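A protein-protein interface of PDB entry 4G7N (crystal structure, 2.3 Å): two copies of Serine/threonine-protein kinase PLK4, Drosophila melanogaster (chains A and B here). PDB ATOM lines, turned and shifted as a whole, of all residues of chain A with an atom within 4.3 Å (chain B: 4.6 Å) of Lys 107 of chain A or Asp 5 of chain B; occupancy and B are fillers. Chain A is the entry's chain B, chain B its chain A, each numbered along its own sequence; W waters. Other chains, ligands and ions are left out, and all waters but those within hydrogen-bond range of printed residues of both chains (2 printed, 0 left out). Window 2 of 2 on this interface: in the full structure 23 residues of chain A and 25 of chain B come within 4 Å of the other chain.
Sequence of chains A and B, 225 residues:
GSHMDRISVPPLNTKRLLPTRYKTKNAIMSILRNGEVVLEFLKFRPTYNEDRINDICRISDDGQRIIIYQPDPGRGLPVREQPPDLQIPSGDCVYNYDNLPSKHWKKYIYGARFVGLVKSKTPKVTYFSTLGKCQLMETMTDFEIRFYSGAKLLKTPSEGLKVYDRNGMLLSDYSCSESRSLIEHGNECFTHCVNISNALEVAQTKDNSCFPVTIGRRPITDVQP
Printed residues of chain B that touch a printed residue of chain A: His 3, Met 4, Asp 5 and Arg 6. Hydrophobic or aromatic side chains of chain B within 4 Å of the printed part of chain A: Met 4. Hydrophobic or aromatic side chains of chain A that line the printed part of chain B: Phe 41 and Tyr 110. Among the printed residues, Asp or Glu carboxylates within 4 Å of a Lys or Arg side-chain nitrogen of the other chain: Lys 107 of chain A with Asp 5 of chain B (2.9 Å).
1 position is printed for both chains. Of the 6 pairs that touch across the chains among the printed residues, none has its exchanged pair printed and touching as well.
The side-chain amino group (NZ) of Lys 107 of chain A lies within salt-bridge range of the side-chain carboxylate (OD1) of Asp 5 of chain B (2.9 Å).
OG of Ser 2 of chain B is in hydrogen-bond range of N of Met 4 of chain B (3.2 Å). OG of Ser 2 of chain B lies close to OD2 of Asp 5 of chain B (3.1 Å). The guanidinium group (NH1) of Arg 6 of chain B sits at hydrogen-bond distance from a ring nitrogen (ND1) of His 3 of chain B (3.3 Å). The backbone carbonyl oxygen (O) of Asp 55 of chain A is in hydrogen-bond range of the backbone NH (N) of Phe 41 of chain A (2.8 Å). The side-chain amino group (NZ) of Lys 107 of chain A is in hydrogen-bond range of a ring nitrogen (ND1) of His 104 of chain A (3.1 Å).
Water W1 lies within hydrogen-bond range of the backbone carbonyl oxygen of Met 4 of chain B (2.6 Å), the backbone carbonyl oxygen of Lys 103 of chain A (2.7 Å) and the side-chain amino group of Lys 107 of chain A (3.2 Å). Water W2 lies within hydrogen-bond range of O of Arg 6 of chain B (3.0 Å), N of Lys 106 of chain A (3.1 Å) and O of Lys 103 of chain A (3.3 Å).
Asp 5 of chain B touches just one residue of chain A: Lys 107. Of the printed residues of chain A, Met 4 of chain B touches Phe 41 (3.6 Å), Lys 106 (3.6 Å) and Tyr 110 (3.9 Å). Of the printed residues of chain B, Phe 41 of chain A touches Met 4. Of the printed residues of chain B, Tyr 110 of chain A touches Met 4 (3.9 Å). Of the printed residues of chain A, His 3 of chain B touches Lys 106. Of the printed residues of chain B, Lys 106 of chain A touches His 3, Met 4 and Arg 6. The nearest printed residue of chain A that does not touch Asp 5 of chain B is Asp 55 of chain A (4.6 Å).
CG of Met 4 of chain B touches CD1 of Phe 41 of chain A, at 3.6 Å. Lys 106 of chain A touches His 3 of chain B. Lys 106 of chain A touches Met 4 of chain B. Lys 106 of chain A touches Arg 6 of chain B. CD1 of Tyr 110 of chain A touches CE of Met 4 of chain B, at 3.9 Å.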
ATOM      1  N   LEU A  39     -32.742 -22.265  25.471  1.00  0.00           N
ATOM      2  CA  LEU A  39     -31.647 -21.329  25.590  1.00  0.00           C
ATOM      3  C   LEU A  39     -31.965 -20.124  24.716  1.00  0.00           C
ATOM      4  O   LEU A  39     -32.154 -20.259  23.507  1.00  0.00           O
ATOM      5  CB  LEU A  39     -30.340 -21.985  25.136  1.00  0.00           C
ATOM      6  CG  LEU A  39     -30.103 -23.401  25.687  1.00  0.00           C
ATOM      7  CD1 LEU A  39     -28.893 -24.036  25.016  1.00  0.00           C
ATOM      8  CD2 LEU A  39     -29.926 -23.368  27.198  1.00  0.00           C
ATOM      9  N   PHE A  41     -30.266 -16.827  23.596  1.00  0.00           N
ATOM     10  CA  PHE A  41     -29.008 -16.088  23.634  1.00  0.00           C
ATOM     11  C   PHE A  41     -29.273 -14.630  23.338  1.00  0.00           C
ATOM     12  O   PHE A  41     -29.995 -14.303  22.400  1.00  0.00           O
ATOM     13  CB  PHE A  41     -27.989 -16.678  22.668  1.00  0.00           C
ATOM     14  CG  PHE A  41     -27.606 -18.080  23.007  1.00  0.00           C
ATOM     15  CD1 PHE A  41     -26.755 -18.341  24.069  1.00  0.00           C
ATOM     16  CD2 PHE A  41     -28.110 -19.145  22.276  1.00  0.00           C
ATOM     17  CE1 PHE A  41     -26.409 -19.645  24.408  1.00  0.00           C
ATOM     18  CE2 PHE A  41     -27.759 -20.442  22.588  1.00  0.00           C
ATOM     19  CZ  PHE A  41     -26.908 -20.696  23.667  1.00  0.00           C
ATOM     20  N   ASP A  55     -30.902 -15.446  19.379  1.00  0.00           N
ATOM     21  CA  ASP A  55     -31.244 -16.760  18.872  1.00  0.00           C
ATOM     22  C   ASP A  55     -31.636 -17.718  19.966  1.00  0.00           C
ATOM     23  O   ASP A  55     -31.370 -17.498  21.152  1.00  0.00           O
ATOM     24  CB  ASP A  55     -30.179 -17.358  17.942  1.00  0.00           C
ATOM     25  CG  ASP A  55     -28.770 -17.175  18.447  1.00  0.00           C
ATOM     26  OD1 ASP A  55     -27.939 -18.067  18.170  1.00  0.00           O
ATOM     27  OD2 ASP A  55     -28.478 -16.148  19.093  1.00  0.00           O
ATOM     28  N   LYS A 103     -21.260 -26.312  13.432  1.00  0.00           N
ATOM     29  CA  LYS A 103     -21.370 -24.888  13.758  1.00  0.00           C
ATOM     30  C   LYS A 103     -22.356 -24.632  14.901  1.00  0.00           C
ATOM     31  O   LYS A 103     -22.410 -23.528  15.449  1.00  0.00           O
ATOM     32  CB  LYS A 103     -21.802 -24.080  12.539  1.00  0.00           C
ATOM     33  CG  LYS A 103     -23.083 -24.599  11.920  1.00  0.00           C
ATOM     34  CD  LYS A 103     -23.873 -23.493  11.235  1.00  0.00           C
ATOM     35  CE  LYS A 103     -25.105 -24.100  10.549  1.00  0.00           C
ATOM     36  NZ  LYS A 103     -26.150 -23.117  10.130  1.00  0.00           N
ATOM     37  N   HIS A 104     -23.133 -25.649  15.253  1.00  0.00           N
ATOM     38  CA  HIS A 104     -24.119 -25.522  16.321  1.00  0.00           C
ATOM     39  C   HIS A 104     -23.697 -26.266  17.583  1.00  0.00           C
ATOM     40  O   HIS A 104     -24.405 -26.252  18.596  1.00  0.00           O
ATOM     41  CB  HIS A 104     -25.472 -26.044  15.839  1.00  0.00           C
ATOM     42  CG  HIS A 104     -26.106 -25.180  14.798  1.00  0.00           C
ATOM     43  ND1 HIS A 104     -26.017 -23.805  14.820  1.00  0.00           N
ATOM     44  CD2 HIS A 104     -26.837 -25.494  13.703  1.00  0.00           C
ATOM     45  CE1 HIS A 104     -26.671 -23.309  13.786  1.00  0.00           C
ATOM     46  NE2 HIS A 104     -27.178 -24.313  13.095  1.00  0.00           N
ATOM     47  N   TRP A 105     -22.554 -26.933  17.519  1.00  0.00           N
ATOM     48  CA  TRP A 105     -22.072 -27.700  18.657  1.00  0.00           C
ATOM     49  C   TRP A 105     -21.859 -26.843  19.907  1.00  0.00           C
ATOM     50  O   TRP A 105     -22.133 -27.290  21.018  1.00  0.00           O
ATOM     51  CB  TRP A 105     -20.787 -28.446  18.297  1.00  0.00           C
ATOM     52  CG  TRP A 105     -21.004 -29.548  17.324  1.00  0.00           C
ATOM     53  CD1 TRP A 105     -22.179 -29.897  16.745  1.00  0.00           C
ATOM     54  CD2 TRP A 105     -20.023 -30.455  16.821  1.00  0.00           C
ATOM     55  NE1 TRP A 105     -21.996 -30.961  15.907  1.00  0.00           N
ATOM     56  CE2 TRP A 105     -20.680 -31.326  15.935  1.00  0.00           C
ATOM     57  CE3 TRP A 105     -18.651 -30.613  17.028  1.00  0.00           C
ATOM     58  CZ2 TRP A 105     -20.016 -32.345  15.259  1.00  0.00           C
ATOM     59  CZ3 TRP A 105     -17.992 -31.623  16.350  1.00  0.00           C
ATOM     60  CH2 TRP A 105     -18.675 -32.474  15.477  1.00  0.00           C
ATOM     61  N   LYS A 106     -21.363 -25.620  19.737  1.00  0.00           N
ATOM     62  CA  LYS A 106     -21.121 -24.760  20.898  1.00  0.00           C
ATOM     63  C   LYS A 106     -22.405 -24.466  21.699  1.00  0.00           C
ATOM     64  O   LYS A 106     -22.397 -24.494  22.935  1.00  0.00           O
ATOM     65  CB  LYS A 106     -20.431 -23.463  20.484  1.00  0.00           C
ATOM     66  CG  LYS A 106     -19.805 -22.697  21.652  1.00  0.00           C
ATOM     67  CD  LYS A 106     -19.053 -21.454  21.159  1.00  0.00           C
ATOM     68  CE  LYS A 106     -18.913 -20.388  22.242  1.00  0.00           C
ATOM     69  NZ  LYS A 106     -17.759 -20.619  23.140  1.00  0.00           N
ATOM     70  N   LYS A 107     -23.497 -24.172  20.993  1.00  0.00           N
ATOM     71  CA  LYS A 107     -24.793 -23.984  21.635  1.00  0.00           C
ATOM     72  C   LYS A 107     -25.229 -25.256  22.384  1.00  0.00           C
ATOM     73  O   LYS A 107     -25.607 -25.210  23.555  1.00  0.00           O
ATOM     74  CB  LYS A 107     -25.863 -23.617  20.603  1.00  0.00           C
ATOM     75  CG  LYS A 107     -25.623 -22.342  19.835  1.00  0.00           C
ATOM     76  CD  LYS A 107     -26.823 -22.047  18.936  1.00  0.00           C
ATOM     77  CE  LYS A 107     -26.479 -21.008  17.867  1.00  0.00           C
ATOM     78  NZ  LYS A 107     -25.512 -21.522  16.842  1.00  0.00           N
ATOM     79  N   TYR A 108     -25.195 -26.391  21.697  1.00  0.00           N
ATOM     80  CA  TYR A 108     -25.594 -27.639  22.324  1.00  0.00           C
ATOM     81  C   TYR A 108     -24.798 -27.916  23.599  1.00  0.00           C
ATOM     82  O   TYR A 108     -25.367 -28.269  24.627  1.00  0.00           O
ATOM     83  CB  TYR A 108     -25.459 -28.810  21.358  1.00  0.00           C
ATOM     84  CG  TYR A 108     -26.083 -30.054  21.931  1.00  0.00           C
ATOM     85  CD1 TYR A 108     -27.377 -30.419  21.587  1.00  0.00           C
ATOM     86  CD2 TYR A 108     -25.389 -30.846  22.837  1.00  0.00           C
ATOM     87  CE1 TYR A 108     -27.966 -31.557  22.123  1.00  0.00           C
ATOM     88  CE2 TYR A 108     -25.963 -31.983  23.387  1.00  0.00           C
ATOM     89  CZ  TYR A 108     -27.254 -32.336  23.019  1.00  0.00           C
ATOM     90  OH  TYR A 108     -27.854 -33.457  23.547  1.00  0.00           O
ATOM     91  N   ILE A 109     -23.484 -27.733  23.531  1.00  0.00           N
ATOM     92  CA  ILE A 109     -22.607 -27.904  24.695  1.00  0.00           C
ATOM     93  C   ILE A 109     -22.947 -26.933  25.827  1.00  0.00           C
ATOM     94  O   ILE A 109     -22.853 -27.266  26.993  1.00  0.00           O
ATOM     95  CB  ILE A 109     -21.156 -27.750  24.281  1.00  0.00           C
ATOM     96  CG1 ILE A 109     -20.705 -29.024  23.552  1.00  0.00           C
ATOM     97  CG2 ILE A 109     -20.274 -27.510  25.479  1.00  0.00           C
ATOM     98  CD1 ILE A 109     -19.479 -28.839  22.647  1.00  0.00           C
ATOM     99  N   TYR A 110     -23.363 -25.728  25.473  1.00  0.00           N
ATOM    100  CA  TYR A 110     -23.829 -24.777  26.471  1.00  0.00           C
ATOM    101  C   TYR A 110     -25.048 -25.358  27.222  1.00  0.00           C
ATOM    102  O   TYR A 110     -25.147 -25.271  28.450  1.00  0.00           O
ATOM    103  CB  TYR A 110     -24.180 -23.469  25.768  1.00  0.00           C
ATOM    104  CG  TYR A 110     -24.431 -22.301  26.683  1.00  0.00           C
ATOM    105  CD1 TYR A 110     -23.427 -21.372  26.938  1.00  0.00           C
ATOM    106  CD2 TYR A 110     -25.676 -22.111  27.282  1.00  0.00           C
ATOM    107  CE1 TYR A 110     -23.642 -20.300  27.779  1.00  0.00           C
ATOM    108  CE2 TYR A 110     -25.901 -21.045  28.114  1.00  0.00           C
ATOM    109  CZ  TYR A 110     -24.879 -20.134  28.363  1.00  0.00           C
ATOM    110  OH  TYR A 110     -25.103 -19.060  29.198  1.00  0.00           O
ATOM    111  N   GLY A 111     -25.971 -25.961  26.472  1.00  0.00           N
ATOM    112  CA  GLY A 111     -27.134 -26.585  27.067  1.00  0.00           C
ATOM    113  C   GLY A 111     -26.750 -27.742  27.985  1.00  0.00           C
ATOM    114  O   GLY A 111     -27.272 -27.860  29.091  1.00  0.00           O
ATOM    115  N   SER B   2     -21.991 -13.432  16.077  1.00  0.00           N
ATOM    116  CA  SER B   2     -22.456 -14.010  17.339  1.00  0.00           C
ATOM    117  C   SER B   2     -21.365 -14.801  18.073  1.00  0.00           C
ATOM    118  O   SER B   2     -20.554 -15.491  17.442  1.00  0.00           O
ATOM    119  CB  SER B   2     -23.691 -14.885  17.102  1.00  0.00           C
ATOM    120  OG  SER B   2     -23.909 -15.778  18.181  1.00  0.00           O
ATOM    121  N   HIS B   3     -21.355 -14.683  19.405  1.00  0.00           N
ATOM    122  CA  HIS B   3     -20.385 -15.364  20.268  1.00  0.00           C
ATOM    123  C   HIS B   3     -20.618 -16.871  20.319  1.00  0.00           C
ATOM    124  O   HIS B   3     -19.700 -17.656  20.539  1.00  0.00           O
ATOM    125  CB  HIS B   3     -20.429 -14.791  21.692  1.00  0.00           C
ATOM    126  CG  HIS B   3     -19.667 -15.600  22.698  1.00  0.00           C
ATOM    127  ND1 HIS B   3     -18.329 -15.910  22.548  1.00  0.00           N
ATOM    128  CD2 HIS B   3     -20.050 -16.165  23.868  1.00  0.00           C
ATOM    129  CE1 HIS B   3     -17.925 -16.630  23.578  1.00  0.00           C
ATOM    130  NE2 HIS B   3     -18.951 -16.800  24.395  1.00  0.00           N
ATOM    131  N   MET B   4     -21.857 -17.284  20.116  1.00  0.00           N
ATOM    132  CA  MET B   4     -22.167 -18.702  20.157  1.00  0.00           C
ATOM    133  C   MET B   4     -21.886 -19.371  18.814  1.00  0.00           C
ATOM    134  O   MET B   4     -21.793 -20.595  18.722  1.00  0.00           O
ATOM    135  CB  MET B   4     -23.602 -18.913  20.619  1.00  0.00           C
ATOM    136  CG  MET B   4     -23.848 -18.342  22.010  1.00  0.00           C
ATOM    137  SD  MET B   4     -22.672 -18.950  23.242  1.00  0.00           S
ATOM    138  CE  MET B   4     -22.979 -20.723  23.158  1.00  0.00           C
ATOM    139  N   ASP B   5     -21.710 -18.550  17.784  1.00  0.00           N
ATOM    140  CA  ASP B   5     -21.334 -19.036  16.466  1.00  0.00           C
ATOM    141  C   ASP B   5     -19.813 -19.024  16.331  1.00  0.00           C
ATOM    142  O   ASP B   5     -19.250 -18.340  15.472  1.00  0.00           O
ATOM    143  CB  ASP B   5     -21.994 -18.176  15.387  1.00  0.00           C
ATOM    144  CG  ASP B   5     -23.508 -18.107  15.548  1.00  0.00           C
ATOM    145  OD1 ASP B   5     -24.126 -19.142  15.892  1.00  0.00           O
ATOM    146  OD2 ASP B   5     -24.082 -17.017  15.342  1.00  0.00           O
ATOM    147  N   ARG B   6     -19.151 -19.781  17.200  1.00  0.00           N
ATOM    148  CA  ARG B   6     -17.702 -19.913  17.157  1.00  0.00           C
ATOM    149  C   ARG B   6     -17.328 -21.371  17.360  1.00  0.00           C
ATOM    150  O   ARG B   6     -18.198 -22.196  17.622  1.00  0.00           O
ATOM    151  CB  ARG B   6     -17.049 -19.018  18.207  1.00  0.00           C
ATOM    152  CG  ARG B   6     -16.967 -17.568  17.771  1.00  0.00           C
ATOM    153  CD  ARG B   6     -16.299 -16.665  18.807  1.00  0.00           C
ATOM    154  NE  ARG B   6     -16.224 -15.292  18.299  1.00  0.00           N
ATOM    155  CZ  ARG B   6     -16.336 -14.193  19.045  1.00  0.00           C
ATOM    156  NH1 ARG B   6     -16.529 -14.286  20.355  1.00  0.00           N
ATOM    157  NH2 ARG B   6     -16.260 -12.996  18.475  1.00  0.00           N
ATOM    158  N   TRP B 105     -13.511 -26.731  11.239  1.00  0.00           N
ATOM    159  CA  TRP B 105     -13.653 -26.904  12.690  1.00  0.00           C
ATOM    160  C   TRP B 105     -13.666 -28.371  13.092  1.00  0.00           C
ATOM    161  O   TRP B 105     -13.076 -28.734  14.115  1.00  0.00           O
ATOM    162  CB  TRP B 105     -14.902 -26.200  13.219  1.00  0.00           C
ATOM    163  CG  TRP B 105     -14.835 -24.712  13.120  1.00  0.00           C
ATOM    164  CD1 TRP B 105     -13.786 -23.969  12.674  1.00  0.00           C
ATOM    165  CD2 TRP B 105     -15.867 -23.778  13.475  1.00  0.00           C
ATOM    166  NE1 TRP B 105     -14.097 -22.626  12.720  1.00  0.00           N
ATOM    167  CE2 TRP B 105     -15.365 -22.482  13.210  1.00  0.00           C
ATOM    168  CE3 TRP B 105     -17.166 -23.914  13.985  1.00  0.00           C
ATOM    169  CZ2 TRP B 105     -16.112 -21.328  13.444  1.00  0.00           C
ATOM    170  CZ3 TRP B 105     -17.909 -22.769  14.212  1.00  0.00           C
ATOM    171  CH2 TRP B 105     -17.378 -21.489  13.945  1.00  0.00           C
HETATM  172  O   HOH W   1     -22.893 -22.886  18.013  1.00  0.00           O
HETATM  173  O   HOH W   2     -19.910 -24.605  17.252  1.00  0.00           O
